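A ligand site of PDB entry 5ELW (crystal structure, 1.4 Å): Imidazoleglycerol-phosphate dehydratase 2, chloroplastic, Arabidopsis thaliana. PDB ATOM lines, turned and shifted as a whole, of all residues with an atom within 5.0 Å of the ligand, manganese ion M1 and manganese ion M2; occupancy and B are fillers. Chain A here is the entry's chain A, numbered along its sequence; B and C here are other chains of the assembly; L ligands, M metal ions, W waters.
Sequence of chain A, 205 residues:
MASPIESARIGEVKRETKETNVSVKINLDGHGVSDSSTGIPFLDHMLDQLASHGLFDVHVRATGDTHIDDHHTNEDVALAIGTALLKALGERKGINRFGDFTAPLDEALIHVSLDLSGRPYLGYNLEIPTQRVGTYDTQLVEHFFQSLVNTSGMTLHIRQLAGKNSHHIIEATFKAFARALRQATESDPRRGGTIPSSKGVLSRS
Residues that only touch the ligand: Ser 198 of chain C.
Within 4 Å of the ligand: His 45, His 167, His 168, Glu 171, Lys 175, Glu 19 of chain B, His 71 of chain B, His 72 of chain B, Glu 75 of chain B, Arg 97 of chain C, Arg 119 of chain C, Ser 197 of chain C, Ser 198 of chain C and Lys 199 of chain C.
Along chain A the residues within 4 Å of the ligand span positions 45 to 175.
O1 of the ligand is in hydrogen-bond range of OG of Ser 197 of chain C (2.6 Å).
NZ of Lys 199 of chain C is in salt-bridge range of O3 of the ligand, at 2.7 Å.
The side-chain amino group (NZ) of Lys 175 is in salt-bridge range of an oxygen (O2) of the ligand.
The side-chain carboxylate of Glu 19 of chain B lies close to an oxygen (O4) of the ligand, 2.8 Å away.
NH1 of Arg 119 of chain C is in salt-bridge range of O3 of the ligand (2.8 Å).
NH1 of Arg 97 of chain C is in salt-bridge range of O1 of the ligand (2.8 Å).
Manganese ion M2 is bound by the side-chain carboxylate (OE1) of Glu 171 (2.1 Å), a ring nitrogen (NE2) of His 45 (2.3 Å), an oxygen (O4) of the ligand (2.3 Å), a nitrogen (N2) of the ligand (2.3 Å), a ring nitrogen (NE2) of His 167 (2.3 Å) and a ring nitrogen (NE2) of His 72 of chain B (2.3 Å).
Manganese ion M2 has six donor atoms within binding distance.
NZ of Lys 175 is in salt-bridge range of OE2 of Glu 171 (2.8 Å).
O of His 45 sits at hydrogen-bond distance from NE2 of Gln 49, 3.3 Å away.
A ring nitrogen (ND1) of His 72 of chain B sits close to the side-chain carboxylate (OE1) of Glu 19 of chain B, at 3.5 Å.
The side-chain hydroxyl (OG) of Ser 197 of chain C sits close to the backbone NH (N) of Lys 199 of chain C, 3.2 Å away.
The guanidinium group (NE) of Arg 119 of chain C lies within salt-bridge range of the side-chain carboxylate (OD1) of Asp 106 (2.9 Å).
The guanidinium group of Arg 97 of chain C lies within hydrogen-bond range of the backbone carbonyl oxygen of Pro 196 of chain C, at 2.9 Å.
The side-chain hydroxyl of Ser 198 of chain C sits at hydrogen-bond distance from the side-chain amide nitrogen of Gln 49, at 3.0 Å.
Manganese ion M1 is bound by water W1 (2.2 Å), the side-chain carboxylate of Glu 75 of chain B (2.2 Å), a nitrogen (N3) of the ligand (2.2 Å), a ring nitrogen (NE2) of His 71 of chain B (2.3 Å), a ring nitrogen (NE2) of His 168 (2.3 Å) and a ring nitrogen (NE2) of His 143 of chain B (2.3 Å).
Within 4 Å of manganese ion M2: His 45, His 167, Glu 171 and His 72 of chain B.
Water W1 lies within hydrogen-bond range of OD2 of Asp 106 (2.6 Å), OE2 of Glu 75 of chain B (2.7 Å) and NE of Arg 119 of chain C (3.4 Å).
Water W2 lies within hydrogen-bond range of O1 of the ligand (2.7 Å), OE1 of Gln 49 (2.7 Å), NE2 of His 53 (2.8 Å) and N of Ser 198 of chain C (2.9 Å).
Of the 22 residues printed, 4 come within 4 Å of manganese ion M1.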
ATOM      1  N   HIS A  45      -2.258 -19.495  16.197  1.00  0.00           N
ATOM      2  CA  HIS A  45      -3.008 -19.841  14.978  1.00  0.00           C
ATOM      3  C   HIS A  45      -2.837 -21.345  14.641  1.00  0.00           C
ATOM      4  O   HIS A  45      -3.773 -22.000  14.205  1.00  0.00           O
ATOM      5  CB  HIS A  45      -2.563 -18.929  13.820  1.00  0.00           C
ATOM      6  CG  HIS A  45      -3.239 -19.187  12.502  1.00  0.00           C
ATOM      7  ND1 HIS A  45      -4.590 -19.357  12.368  1.00  0.00           N
ATOM      8  CD2 HIS A  45      -2.722 -19.278  11.247  1.00  0.00           C
ATOM      9  CE1 HIS A  45      -4.887 -19.568  11.098  1.00  0.00           C
ATOM     10  NE2 HIS A  45      -3.779 -19.510  10.391  1.00  0.00           N
ATOM     11  N   MET A  46      -1.632 -21.846  14.851  1.00  0.00           N
ATOM     12  CA  MET A  46      -1.356 -23.279  14.589  1.00  0.00           C
ATOM     13  C   MET A  46      -2.066 -24.156  15.619  1.00  0.00           C
ATOM     14  O   MET A  46      -2.627 -25.200  15.271  1.00  0.00           O
ATOM     15  CB  MET A  46       0.160 -23.546  14.616  1.00  0.00           C
ATOM     16  CG  MET A  46       0.919 -22.864  13.498  1.00  0.00           C
ATOM     17  SD  MET A  46       0.304 -23.293  11.832  1.00  0.00           S
ATOM     18  CE  MET A  46      -0.729 -21.868  11.485  1.00  0.00           C
ATOM     19  N   GLN A  49      -5.556 -24.809  14.773  1.00  0.00           N
ATOM     20  CA  GLN A  49      -5.773 -25.929  13.836  1.00  0.00           C
ATOM     21  C   GLN A  49      -5.809 -27.274  14.565  1.00  0.00           C
ATOM     22  O   GLN A  49      -6.545 -28.163  14.215  1.00  0.00           O
ATOM     23  CB  GLN A  49      -4.698 -25.970  12.749  1.00  0.00           C
ATOM     24  CG  GLN A  49      -4.503 -24.660  12.016  1.00  0.00           C
ATOM     25  CD  GLN A  49      -5.793 -24.026  11.570  1.00  0.00           C
ATOM     26  OE1 GLN A  49      -6.631 -24.666  10.914  1.00  0.00           O
ATOM     27  NE2 GLN A  49      -5.983 -22.781  11.914  1.00  0.00           N
ATOM     28  N   HIS A  53      -9.225 -29.206  13.844  1.00  0.00           N
ATOM     29  CA  HIS A  53      -9.114 -30.413  13.006  1.00  0.00           C
ATOM     30  C   HIS A  53      -8.889 -31.687  13.799  1.00  0.00           C
ATOM     31  O   HIS A  53      -9.352 -32.754  13.385  1.00  0.00           O
ATOM     32  CB  HIS A  53      -8.099 -30.186  11.904  1.00  0.00           C
ATOM     33  CG  HIS A  53      -8.557 -29.108  10.989  1.00  0.00           C
ATOM     34  ND1 HIS A  53      -9.688 -29.246  10.208  1.00  0.00           N
ATOM     35  CD2 HIS A  53      -8.181 -27.817  10.856  1.00  0.00           C
ATOM     36  CE1 HIS A  53      -9.954 -28.107   9.605  1.00  0.00           C
ATOM     37  NE2 HIS A  53      -9.039 -27.225   9.971  1.00  0.00           N
ATOM     38  N   LEU A 105      -2.327 -27.703   2.104  1.00  0.00           N
ATOM     39  CA  LEU A 105      -2.837 -26.339   2.159  1.00  0.00           C
ATOM     40  C   LEU A 105      -2.343 -25.739   0.857  1.00  0.00           C
ATOM     41  O   LEU A 105      -1.173 -25.439   0.698  1.00  0.00           O
ATOM     42  CB  LEU A 105      -2.404 -25.530   3.389  1.00  0.00           C
ATOM     43  CG  LEU A 105      -3.375 -24.348   3.668  1.00  0.00           C
ATOM     44  CD1 LEU A 105      -2.897 -23.558   4.886  1.00  0.00           C
ATOM     45  CD2 LEU A 105      -3.553 -23.394   2.492  1.00  0.00           C
ATOM     46  N   ASP A 106      -3.265 -25.667  -0.097  1.00  0.00           N
ATOM     47  CA  ASP A 106      -2.959 -25.228  -1.426  1.00  0.00           C
ATOM     48  C   ASP A 106      -1.803 -26.079  -2.005  1.00  0.00           C
ATOM     49  O   ASP A 106      -1.912 -27.313  -2.084  1.00  0.00           O
ATOM     50  CB  ASP A 106      -2.712 -23.720  -1.524  1.00  0.00           C
ATOM     51  CG  ASP A 106      -3.947 -22.895  -1.160  1.00  0.00           C
ATOM     52  OD1 ASP A 106      -5.018 -23.480  -0.875  1.00  0.00           O
ATOM     53  OD2 ASP A 106      -3.821 -21.659  -1.183  1.00  0.00           O
ATOM     54  N   HIS A 167       3.916 -20.233   5.420  1.00  0.00           N
ATOM     55  CA  HIS A 167       2.680 -20.333   6.218  1.00  0.00           C
ATOM     56  C   HIS A 167       1.905 -21.605   5.793  1.00  0.00           C
ATOM     57  O   HIS A 167       1.439 -22.386   6.635  1.00  0.00           O
ATOM     58  CB  HIS A 167       1.887 -19.021   6.043  1.00  0.00           C
ATOM     59  CG  HIS A 167       0.590 -18.889   6.799  1.00  0.00           C
ATOM     60  ND1 HIS A 167       0.178 -17.677   7.300  1.00  0.00           N
ATOM     61  CD2 HIS A 167      -0.446 -19.745   7.016  1.00  0.00           C
ATOM     62  CE1 HIS A 167      -1.022 -17.791   7.831  1.00  0.00           C
ATOM     63  NE2 HIS A 167      -1.436 -19.035   7.656  1.00  0.00           N
ATOM     64  N   HIS A 168       1.794 -21.853   4.492  1.00  0.00           N
ATOM     65  CA  HIS A 168       1.120 -23.088   4.009  1.00  0.00           C
ATOM     66  C   HIS A 168       1.804 -24.373   4.496  1.00  0.00           C
ATOM     67  O   HIS A 168       1.156 -25.303   4.960  1.00  0.00           O
ATOM     68  CB  HIS A 168       1.025 -23.106   2.498  1.00  0.00           C
ATOM     69  CG  HIS A 168       0.092 -22.086   1.929  1.00  0.00           C
ATOM     70  ND1 HIS A 168      -0.081 -21.937   0.577  1.00  0.00           N
ATOM     71  CD2 HIS A 168      -0.711 -21.182   2.512  1.00  0.00           C
ATOM     72  CE1 HIS A 168      -0.968 -20.982   0.356  1.00  0.00           C
ATOM     73  NE2 HIS A 168      -1.370 -20.504   1.511  1.00  0.00           N
ATOM     74  N   GLU A 171       1.272 -24.669   8.350  1.00  0.00           N
ATOM     75  CA  GLU A 171      -0.122 -24.886   8.706  1.00  0.00           C
ATOM     76  C   GLU A 171      -0.600 -26.270   8.250  1.00  0.00           C
ATOM     77  O   GLU A 171      -1.317 -26.976   8.984  1.00  0.00           O
ATOM     78  CB  GLU A 171      -1.018 -23.784   8.161  1.00  0.00           C
ATOM     79  CG  GLU A 171      -2.430 -23.904   8.682  1.00  0.00           C
ATOM     80  CD  GLU A 171      -3.326 -22.777   8.258  1.00  0.00           C
ATOM     81  OE1 GLU A 171      -2.841 -21.633   8.167  1.00  0.00           O
ATOM     82  OE2 GLU A 171      -4.520 -23.060   7.987  1.00  0.00           O
ATOM     83  N   LYS A 175      -2.216 -29.226  10.539  1.00  0.00           N
ATOM     84  CA  LYS A 175      -3.470 -29.903  10.174  1.00  0.00           C
ATOM     85  C   LYS A 175      -3.282 -31.425  10.082  1.00  0.00           C
ATOM     86  O   LYS A 175      -4.095 -32.189  10.605  1.00  0.00           O
ATOM     87  CB  LYS A 175      -4.020 -29.332   8.877  1.00  0.00           C
ATOM     88  CG  LYS A 175      -4.697 -27.981   9.062  1.00  0.00           C
ATOM     89  CD  LYS A 175      -4.880 -27.229   7.748  1.00  0.00           C
ATOM     90  CE  LYS A 175      -5.894 -26.098   7.867  1.00  0.00           C
ATOM     91  NZ  LYS A 175      -5.746 -25.176   6.699  1.00  0.00           N
ATOM     92  N   GLU B  19     -10.840 -14.143  10.071  1.00  0.00           N
ATOM     93  CA  GLU B  19      -9.472 -13.644   9.877  1.00  0.00           C
ATOM     94  C   GLU B  19      -9.386 -12.207   9.386  1.00  0.00           C
ATOM     95  O   GLU B  19      -8.474 -11.458   9.755  1.00  0.00           O
ATOM     96  CB  GLU B  19      -8.695 -14.545   8.894  1.00  0.00           C
ATOM     97  CG  GLU B  19      -8.564 -15.997   9.373  1.00  0.00           C
ATOM     98  CD  GLU B  19      -8.030 -16.979   8.319  1.00  0.00           C
ATOM     99  OE1 GLU B  19      -8.029 -16.660   7.106  1.00  0.00           O
ATOM    100  OE2 GLU B  19      -7.629 -18.099   8.761  1.00  0.00           O
ATOM    101  N   HIS B  71      -0.478 -12.600   5.616  1.00  0.00           N
ATOM    102  CA  HIS B  71      -0.942 -13.603   4.678  1.00  0.00           C
ATOM    103  C   HIS B  71      -2.457 -13.583   4.433  1.00  0.00           C
ATOM    104  O   HIS B  71      -2.890 -13.481   3.273  1.00  0.00           O
ATOM    105  CB  HIS B  71      -0.540 -14.983   5.177  1.00  0.00           C
ATOM    106  CG  HIS B  71      -0.802 -16.092   4.211  1.00  0.00           C
ATOM    107  ND1 HIS B  71       0.213 -16.878   3.719  1.00  0.00           N
ATOM    108  CD2 HIS B  71      -1.941 -16.574   3.682  1.00  0.00           C
ATOM    109  CE1 HIS B  71      -0.275 -17.796   2.919  1.00  0.00           C
ATOM    110  NE2 HIS B  71      -1.590 -17.642   2.871  1.00  0.00           N
ATOM    111  N   HIS B  72      -3.234 -13.726   5.501  1.00  0.00           N
ATOM    112  CA  HIS B  72      -4.688 -13.820   5.307  1.00  0.00           C
ATOM    113  C   HIS B  72      -5.241 -12.553   4.662  1.00  0.00           C
ATOM    114  O   HIS B  72      -6.080 -12.604   3.786  1.00  0.00           O
ATOM    115  CB  HIS B  72      -5.437 -14.131   6.604  1.00  0.00           C
ATOM    116  CG  HIS B  72      -4.999 -15.402   7.296  1.00  0.00           C
ATOM    117  ND1 HIS B  72      -5.128 -15.587   8.647  1.00  0.00           N
ATOM    118  CD2 HIS B  72      -4.455 -16.560   6.825  1.00  0.00           C
ATOM    119  CE1 HIS B  72      -4.686 -16.780   9.000  1.00  0.00           C
ATOM    120  NE2 HIS B  72      -4.290 -17.397   7.902  1.00  0.00           N
ATOM    121  N   GLU B  75      -4.235 -12.410   0.925  1.00  0.00           N
ATOM    122  CA  GLU B  75      -5.027 -13.411   0.221  1.00  0.00           C
ATOM    123  C   GLU B  75      -6.465 -12.958  -0.005  1.00  0.00           C
ATOM    124  O   GLU B  75      -7.010 -13.069  -1.112  1.00  0.00           O
ATOM    125  CB  GLU B  75      -4.994 -14.738   0.986  1.00  0.00           C
ATOM    126  CG  GLU B  75      -5.909 -15.808   0.422  1.00  0.00           C
ATOM    127  CD  GLU B  75      -5.598 -17.209   0.906  1.00  0.00           C
ATOM    128  OE1 GLU B  75      -4.593 -17.371   1.655  1.00  0.00           O
ATOM    129  OE2 GLU B  75      -6.346 -18.153   0.537  1.00  0.00           O
ATOM    130  N   HIS B 143       1.091 -15.251  -4.158  1.00  0.00           N
ATOM    131  CA  HIS B 143      -0.210 -15.606  -3.603  1.00  0.00           C
ATOM    132  C   HIS B 143      -1.271 -14.596  -3.984  1.00  0.00           C
ATOM    133  O   HIS B 143      -2.437 -14.965  -4.224  1.00  0.00           O
ATOM    134  CB  HIS B 143      -0.130 -15.729  -2.105  1.00  0.00           C
ATOM    135  CG  HIS B 143      -1.189 -16.600  -1.498  1.00  0.00           C
ATOM    136  ND1 HIS B 143      -2.484 -16.651  -1.957  1.00  0.00           N
ATOM    137  CD2 HIS B 143      -1.112 -17.481  -0.476  1.00  0.00           C
ATOM    138  CE1 HIS B 143      -3.165 -17.508  -1.219  1.00  0.00           C
ATOM    139  NE2 HIS B 143      -2.361 -18.017  -0.314  1.00  0.00           N
ATOM    140  N   ARG C  97     -13.858 -32.914   5.452  1.00  0.00           N
ATOM    141  CA  ARG C  97     -13.151 -31.862   4.680  1.00  0.00           C
ATOM    142  C   ARG C  97     -11.920 -32.358   3.939  1.00  0.00           C
ATOM    143  O   ARG C  97     -11.724 -32.043   2.750  1.00  0.00           O
ATOM    144  CB  ARG C  97     -12.806 -30.649   5.569  1.00  0.00           C
ATOM    145  CG  ARG C  97     -12.012 -29.590   4.825  1.00  0.00           C
ATOM    146  CD  ARG C  97     -11.613 -28.408   5.690  1.00  0.00           C
ATOM    147  NE  ARG C  97     -10.599 -27.615   5.031  1.00  0.00           N
ATOM    148  CZ  ARG C  97     -10.063 -26.507   5.507  1.00  0.00           C
ATOM    149  NH1 ARG C  97     -10.486 -25.962   6.626  1.00  0.00           N
ATOM    150  NH2 ARG C  97      -9.096 -25.908   4.832  1.00  0.00           N
ATOM    151  N   ARG C 119     -10.653 -23.571  -2.214  1.00  0.00           N
ATOM    152  CA  ARG C 119      -9.555 -22.957  -2.950  1.00  0.00           C
ATOM    153  C   ARG C 119      -9.027 -23.927  -4.021  1.00  0.00           C
ATOM    154  O   ARG C 119      -8.491 -24.982  -3.673  1.00  0.00           O
ATOM    155  CB  ARG C 119      -8.423 -22.617  -2.001  1.00  0.00           C
ATOM    156  CG  ARG C 119      -8.752 -21.643  -0.895  1.00  0.00           C
ATOM    157  CD  ARG C 119      -7.535 -21.301  -0.046  1.00  0.00           C
ATOM    158  NE  ARG C 119      -7.152 -22.397   0.847  1.00  0.00           N
ATOM    159  CZ  ARG C 119      -7.509 -22.514   2.116  1.00  0.00           C
ATOM    160  NH1 ARG C 119      -8.252 -21.588   2.706  1.00  0.00           N
ATOM    161  NH2 ARG C 119      -7.129 -23.566   2.813  1.00  0.00           N
ATOM    162  N   PRO C 196     -15.908 -27.035   9.282  1.00  0.00           N
ATOM    163  CA  PRO C 196     -14.576 -27.473   9.639  1.00  0.00           C
ATOM    164  C   PRO C 196     -13.487 -26.504   9.150  1.00  0.00           C
ATOM    165  O   PRO C 196     -12.659 -26.830   8.281  1.00  0.00           O
ATOM    166  CB  PRO C 196     -14.471 -28.836   8.958  1.00  0.00           C
ATOM    167  CG  PRO C 196     -15.342 -28.686   7.753  1.00  0.00           C
ATOM    168  CD  PRO C 196     -16.487 -27.845   8.202  1.00  0.00           C
ATOM    169  N   SER C 197     -13.485 -25.322   9.757  1.00  0.00           N
ATOM    170  CA  SER C 197     -12.527 -24.285   9.423  1.00  0.00           C
ATOM    171  C   SER C 197     -12.392 -23.324  10.575  1.00  0.00           C
ATOM    172  O   SER C 197     -13.392 -22.796  11.053  1.00  0.00           O
ATOM    173  CB  SER C 197     -12.957 -23.495   8.189  1.00  0.00           C
ATOM    174  OG  SER C 197     -12.058 -22.425   7.955  1.00  0.00           O
ATOM    175  N   SER C 198     -11.152 -23.034  10.956  1.00  0.00           N
ATOM    176  CA  SER C 198     -10.900 -22.034  11.995  1.00  0.00           C
ATOM    177  C   SER C 198     -11.364 -20.637  11.609  1.00  0.00           C
ATOM    178  O   SER C 198     -11.604 -19.808  12.478  1.00  0.00           O
ATOM    179  CB  SER C 198      -9.425 -22.016  12.366  1.00  0.00           C
ATOM    180  OG  SER C 198      -8.627 -21.644  11.257  1.00  0.00           O
ATOM    181  N   LYS C 199     -11.505 -20.354  10.307  1.00  0.00           N
ATOM    182  CA  LYS C 199     -11.951 -19.019   9.870  1.00  0.00           C
ATOM    183  C   LYS C 199     -13.480 -18.888   9.777  1.00  0.00           C
ATOM    184  O   LYS C 199     -13.988 -17.811   9.477  1.00  0.00           O
ATOM    185  CB  LYS C 199     -11.281 -18.574   8.569  1.00  0.00           C
ATOM    186  CG  LYS C 199     -11.796 -19.229   7.312  1.00  0.00           C
ATOM    187  CD  LYS C 199     -11.011 -18.805   6.091  1.00  0.00           C
ATOM    188  CE  LYS C 199     -11.630 -19.304   4.804  1.00  0.00           C
ATOM    189  NZ  LYS C 199     -11.727 -20.775   4.749  1.00  0.00           N
ATOM    190  N   LEU C 202     -16.193 -21.876   4.610  1.00  0.00           N
ATOM    191  CA  LEU C 202     -15.454 -22.471   3.461  1.00  0.00           C
ATOM    192  C   LEU C 202     -16.149 -21.983   2.220  1.00  0.00           C
ATOM    193  O   LEU C 202     -17.374 -22.115   2.113  1.00  0.00           O
ATOM    194  CB  LEU C 202     -15.463 -23.997   3.532  1.00  0.00           C
ATOM    195  CG  LEU C 202     -14.594 -24.579   4.661  1.00  0.00           C
ATOM    196  CD1 LEU C 202     -14.851 -26.088   4.801  1.00  0.00           C
ATOM    197  CD2 LEU C 202     -13.103 -24.328   4.459  1.00  0.00           C
HETATM  198  O1  LIG L   1      -9.673 -23.324   7.249  1.00  0.00           O
HETATM  199  P1  LIG L   1      -8.674 -22.592   6.380  1.00  0.00           P
HETATM  200  O2  LIG L   1      -7.681 -23.562   5.751  1.00  0.00           O
HETATM  201  O3  LIG L   1      -9.277 -21.727   5.312  1.00  0.00           O
HETATM  202  C1  LIG L   1      -7.794 -21.519   7.552  1.00  0.00           C
HETATM  203  C2  LIG L   1      -6.484 -20.898   7.071  1.00  0.00           C
HETATM  204  O4  LIG L   1      -5.861 -20.187   8.157  1.00  0.00           O
HETATM  205  C3  LIG L   1      -6.615 -19.910   5.945  1.00  0.00           C
HETATM  206  N1  LIG L   1      -5.363 -19.776   5.189  1.00  0.00           N
HETATM  207  N2  LIG L   1      -4.143 -19.715   5.857  1.00  0.00           N
HETATM  208  C4  LIG L   1      -3.239 -19.554   4.869  1.00  0.00           C
HETATM  209  N3  LIG L   1      -3.850 -19.509   3.679  1.00  0.00           N
HETATM  210  C5  LIG L   1      -5.161 -19.660   3.884  1.00  0.00           C
HETATM  211 MN    MN M   1      -3.011 -18.938   1.675  1.00  0.00          MN
HETATM  212 MN    MN M   2      -3.646 -19.643   8.130  1.00  0.00          MN
HETATM  213  O   HOH W   1      -4.611 -20.155   0.832  1.00  0.00           O
HETATM  214  O   HOH W   2      -9.022 -24.442   9.584  1.00  0.00           O
